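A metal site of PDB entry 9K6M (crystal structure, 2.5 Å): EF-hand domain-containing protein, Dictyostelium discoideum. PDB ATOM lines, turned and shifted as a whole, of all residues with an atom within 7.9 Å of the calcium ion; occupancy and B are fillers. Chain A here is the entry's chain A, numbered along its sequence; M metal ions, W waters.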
ATOM      1  N   LYS A  55      13.060 -32.333  26.613  1.00  0.00           N
ATOM      2  CA  LYS A  55      12.161 -32.626  27.708  1.00  0.00           C
ATOM      3  C   LYS A  55      11.366 -33.868  27.307  1.00  0.00           C
ATOM      4  O   LYS A  55      10.673 -33.844  26.294  1.00  0.00           O
ATOM      5  CB  LYS A  55      11.320 -31.392  28.042  1.00  0.00           C
ATOM      6  CG  LYS A  55      10.379 -31.538  29.236  1.00  0.00           C
ATOM      7  CD  LYS A  55       9.610 -30.275  29.598  1.00  0.00           C
ATOM      8  CE  LYS A  55       8.710 -29.786  28.480  1.00  0.00           C
ATOM      9  NZ  LYS A  55       7.960 -28.547  28.827  1.00  0.00           N
ATOM     10  N   PHE A  60      13.216 -28.779  22.117  1.00  0.00           N
ATOM     11  CA  PHE A  60      12.540 -27.540  22.429  1.00  0.00           C
ATOM     12  C   PHE A  60      13.499 -26.345  22.334  1.00  0.00           C
ATOM     13  O   PHE A  60      14.712 -26.501  22.457  1.00  0.00           O
ATOM     14  CB  PHE A  60      11.962 -27.608  23.840  1.00  0.00           C
ATOM     15  CG  PHE A  60      10.770 -28.505  24.050  1.00  0.00           C
ATOM     16  CD1 PHE A  60       9.486 -28.031  23.867  1.00  0.00           C
ATOM     17  CD2 PHE A  60      10.939 -29.816  24.460  1.00  0.00           C
ATOM     18  CE1 PHE A  60       8.384 -28.841  24.084  1.00  0.00           C
ATOM     19  CE2 PHE A  60       9.842 -30.628  24.697  1.00  0.00           C
ATOM     20  CZ  PHE A  60       8.569 -30.150  24.502  1.00  0.00           C
ATOM     21  N   MET A  61      12.920 -25.159  22.183  1.00  0.00           N
ATOM     22  CA  MET A  61      13.631 -23.898  22.082  1.00  0.00           C
ATOM     23  C   MET A  61      13.378 -23.062  23.347  1.00  0.00           C
ATOM     24  O   MET A  61      12.245 -22.885  23.760  1.00  0.00           O
ATOM     25  CB  MET A  61      13.084 -23.099  20.900  1.00  0.00           C
ATOM     26  CG  MET A  61      13.623 -23.470  19.543  1.00  0.00           C
ATOM     27  SD  MET A  61      12.844 -22.409  18.270  1.00  0.00           S
ATOM     28  CE  MET A  61      13.817 -22.881  16.840  1.00  0.00           C
ATOM     29  N   PHE A  97       7.522 -14.238  21.009  1.00  0.00           N
ATOM     30  CA  PHE A  97       7.684 -15.439  21.806  1.00  0.00           C
ATOM     31  C   PHE A  97       6.370 -15.779  22.482  1.00  0.00           C
ATOM     32  O   PHE A  97       5.936 -16.919  22.483  1.00  0.00           O
ATOM     33  CB  PHE A  97       8.825 -15.320  22.828  1.00  0.00           C
ATOM     34  CG  PHE A  97       9.043 -16.617  23.557  1.00  0.00           C
ATOM     35  CD1 PHE A  97       8.339 -16.906  24.705  1.00  0.00           C
ATOM     36  CD2 PHE A  97       9.870 -17.586  23.037  1.00  0.00           C
ATOM     37  CE1 PHE A  97       8.486 -18.131  25.350  1.00  0.00           C
ATOM     38  CE2 PHE A  97      10.016 -18.797  23.693  1.00  0.00           C
ATOM     39  CZ  PHE A  97       9.314 -19.077  24.831  1.00  0.00           C
ATOM     40  N   ALA A 100       4.294 -17.277  19.770  1.00  0.00           N
ATOM     41  CA  ALA A 100       4.717 -18.583  19.322  1.00  0.00           C
ATOM     42  C   ALA A 100       4.454 -19.678  20.375  1.00  0.00           C
ATOM     43  O   ALA A 100       4.185 -20.812  19.995  1.00  0.00           O
ATOM     44  CB  ALA A 100       6.168 -18.514  18.960  1.00  0.00           C
ATOM     45  N   ASP A 101       4.487 -19.325  21.666  1.00  0.00           N
ATOM     46  CA  ASP A 101       4.351 -20.283  22.752  1.00  0.00           C
ATOM     47  C   ASP A 101       2.881 -20.465  23.172  1.00  0.00           C
ATOM     48  O   ASP A 101       2.442 -19.940  24.201  1.00  0.00           O
ATOM     49  CB  ASP A 101       5.203 -19.875  23.972  1.00  0.00           C
ATOM     50  CG  ASP A 101       5.097 -20.822  25.155  1.00  0.00           C
ATOM     51  OD1 ASP A 101       5.021 -22.050  24.925  1.00  0.00           O
ATOM     52  OD2 ASP A 101       5.121 -20.332  26.313  1.00  0.00           O
ATOM     53  N   VAL A 102       2.161 -21.285  22.402  1.00  0.00           N
ATOM     54  CA  VAL A 102       0.724 -21.422  22.542  1.00  0.00           C
ATOM     55  C   VAL A 102       0.359 -22.053  23.887  1.00  0.00           C
ATOM     56  O   VAL A 102      -0.507 -21.538  24.604  1.00  0.00           O
ATOM     57  CB  VAL A 102       0.187 -22.249  21.356  1.00  0.00           C
ATOM     58  CG1 VAL A 102      -1.266 -22.665  21.544  1.00  0.00           C
ATOM     59  CG2 VAL A 102       0.399 -21.502  20.028  1.00  0.00           C
ATOM     60  N   ASP A 103       1.023 -23.148  24.261  1.00  0.00           N
ATOM     61  CA  ASP A 103       0.685 -23.884  25.483  1.00  0.00           C
ATOM     62  C   ASP A 103       1.118 -23.109  26.718  1.00  0.00           C
ATOM     63  O   ASP A 103       0.502 -23.271  27.763  1.00  0.00           O
ATOM     64  CB  ASP A 103       1.245 -25.314  25.480  1.00  0.00           C
ATOM     65  CG  ASP A 103       2.751 -25.465  25.310  1.00  0.00           C
ATOM     66  OD1 ASP A 103       3.468 -24.451  25.417  1.00  0.00           O
ATOM     67  OD2 ASP A 103       3.194 -26.596  25.052  1.00  0.00           O
ATOM     68  N   GLY A 104       2.166 -22.281  26.635  1.00  0.00           N
ATOM     69  CA  GLY A 104       2.533 -21.405  27.736  1.00  0.00           C
ATOM     70  C   GLY A 104       3.558 -21.989  28.720  1.00  0.00           C
ATOM     71  O   GLY A 104       3.739 -21.480  29.827  1.00  0.00           O
ATOM     72  N   ASP A 105       4.276 -23.038  28.299  1.00  0.00           N
ATOM     73  CA  ASP A 105       5.302 -23.644  29.140  1.00  0.00           C
ATOM     74  C   ASP A 105       6.600 -22.860  29.065  1.00  0.00           C
ATOM     75  O   ASP A 105       7.577 -23.251  29.703  1.00  0.00           O
ATOM     76  CB  ASP A 105       5.535 -25.122  28.792  1.00  0.00           C
ATOM     77  CG  ASP A 105       5.867 -25.400  27.329  1.00  0.00           C
ATOM     78  OD1 ASP A 105       6.229 -24.435  26.627  1.00  0.00           O
ATOM     79  OD2 ASP A 105       5.736 -26.584  26.908  1.00  0.00           O
ATOM     80  N   GLY A 106       6.625 -21.757  28.296  1.00  0.00           N
ATOM     81  CA  GLY A 106       7.826 -20.941  28.182  1.00  0.00           C
ATOM     82  C   GLY A 106       8.903 -21.579  27.314  1.00  0.00           C
ATOM     83  O   GLY A 106      10.059 -21.135  27.361  1.00  0.00           O
ATOM     84  N   LEU A 107       8.523 -22.583  26.484  1.00  0.00           N
ATOM     85  CA  LEU A 107       9.397 -23.190  25.485  1.00  0.00           C
ATOM     86  C   LEU A 107       8.683 -23.268  24.143  1.00  0.00           C
ATOM     87  O   LEU A 107       7.469 -23.411  24.084  1.00  0.00           O
ATOM     88  CB  LEU A 107       9.790 -24.597  25.926  1.00  0.00           C
ATOM     89  CG  LEU A 107      10.636 -24.707  27.200  1.00  0.00           C
ATOM     90  CD1 LEU A 107      10.949 -26.156  27.512  1.00  0.00           C
ATOM     91  CD2 LEU A 107      11.915 -23.928  27.057  1.00  0.00           C
ATOM     92  N   ILE A 108       9.431 -23.200  23.045  1.00  0.00           N
ATOM     93  CA  ILE A 108       8.833 -23.334  21.728  1.00  0.00           C
ATOM     94  C   ILE A 108       9.041 -24.769  21.265  1.00  0.00           C
ATOM     95  O   ILE A 108      10.156 -25.246  21.093  1.00  0.00           O
ATOM     96  CB  ILE A 108       9.408 -22.317  20.730  1.00  0.00           C
ATOM     97  CG1 ILE A 108       9.425 -20.894  21.269  1.00  0.00           C
ATOM     98  CG2 ILE A 108       8.659 -22.384  19.416  1.00  0.00           C
ATOM     99  CD1 ILE A 108       8.075 -20.334  21.647  1.00  0.00           C
ATOM    100  N   SER A 109       7.930 -25.462  21.041  1.00  0.00           N
ATOM    101  CA  SER A 109       7.959 -26.808  20.497  1.00  0.00           C
ATOM    102  C   SER A 109       8.262 -26.731  19.009  1.00  0.00           C
ATOM    103  O   SER A 109       8.253 -25.655  18.420  1.00  0.00           O
ATOM    104  CB  SER A 109       6.661 -27.555  20.778  1.00  0.00           C
ATOM    105  OG  SER A 109       5.590 -27.108  19.958  1.00  0.00           O
ATOM    106  N   PHE A 110       8.570 -27.884  18.440  1.00  0.00           N
ATOM    107  CA  PHE A 110       8.651 -28.011  16.996  1.00  0.00           C
ATOM    108  C   PHE A 110       7.348 -27.530  16.368  1.00  0.00           C
ATOM    109  O   PHE A 110       7.366 -26.712  15.451  1.00  0.00           O
ATOM    110  CB  PHE A 110       8.924 -29.469  16.611  1.00  0.00           C
ATOM    111  CG  PHE A 110       8.844 -29.711  15.141  1.00  0.00           C
ATOM    112  CD1 PHE A 110       7.618 -29.929  14.519  1.00  0.00           C
ATOM    113  CD2 PHE A 110       9.982 -29.693  14.350  1.00  0.00           C
ATOM    114  CE1 PHE A 110       7.552 -30.150  13.150  1.00  0.00           C
ATOM    115  CE2 PHE A 110       9.916 -29.914  12.981  1.00  0.00           C
ATOM    116  CZ  PHE A 110       8.699 -30.147  12.386  1.00  0.00           C
ATOM    117  N   GLU A 112       5.032 -25.529  17.526  1.00  0.00           N
ATOM    118  CA  GLU A 112       4.914 -24.084  17.695  1.00  0.00           C
ATOM    119  C   GLU A 112       5.841 -23.332  16.744  1.00  0.00           C
ATOM    120  O   GLU A 112       5.483 -22.275  16.244  1.00  0.00           O
ATOM    121  CB  GLU A 112       5.192 -23.727  19.152  1.00  0.00           C
ATOM    122  CG  GLU A 112       4.176 -24.297  20.112  1.00  0.00           C
ATOM    123  CD  GLU A 112       4.513 -24.125  21.586  1.00  0.00           C
ATOM    124  OE1 GLU A 112       5.689 -23.954  21.920  1.00  0.00           O
ATOM    125  OE2 GLU A 112       3.578 -24.112  22.400  1.00  0.00           O
ATOM    126  N   LEU A 151      -1.931 -26.541  14.586  1.00  0.00           N
ATOM    127  CA  LEU A 151      -0.879 -26.804  15.564  1.00  0.00           C
ATOM    128  C   LEU A 151      -0.749 -28.296  15.870  1.00  0.00           C
ATOM    129  O   LEU A 151       0.358 -28.818  15.830  1.00  0.00           O
ATOM    130  CB  LEU A 151      -1.189 -26.003  16.828  1.00  0.00           C
ATOM    131  CG  LEU A 151      -0.128 -26.101  17.915  1.00  0.00           C
ATOM    132  CD1 LEU A 151       1.234 -25.628  17.401  1.00  0.00           C
ATOM    133  CD2 LEU A 151      -0.553 -25.293  19.132  1.00  0.00           C
HETATM  134 CA    CA M   1       5.265 -24.091  24.256  1.00  0.00          CA
HETATM  135  O   HOH W   1       5.818 -26.782  24.346  1.00  0.00           O
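The backbone NH of Gly 106 lies within hydrogen-bond range of the side-chain carboxylate of Asp 101, at 2.9 Å.
The side-chain carboxylate of Asp 105 lies within salt-bridge range of the side-chain amino group of Lys 55 (3.5 Å).
OG of Ser 109 sits at hydrogen-bond distance from N of Glu 112 (3.0 Å).
The side-chain carboxylate of Asp 101 sits close to the backbone NH of Gly 104 (3.3 Å).
The side-chain carboxylate (OE2) of Glu 112 sits close to the backbone NH (N) of Val 102.
Within 4 Å of the calcium ion: Asp 101, Asp 103, Asp 105, Leu 107 and Glu 112.
The calcium ion is bound by the side-chain carboxylate (OD1) of Asp 101 (2.2 Å), the side-chain carboxylate (OD1) of Asp 103 (2.2 Å), the backbone carbonyl oxygen (O) of Leu 107 (2.3 Å), the side-chain carboxylate (OE1) of Glu 112 (2.4 Å), the side-chain carboxylate (OE2) of Glu 112 (2.5 Å), the side-chain carboxylate (OD1) of Asp 105 (2.6 Å) and water W1 (2.7 Å).
Water W1 bridges OD2 of Asp 105 and OD2 of Asp 103.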
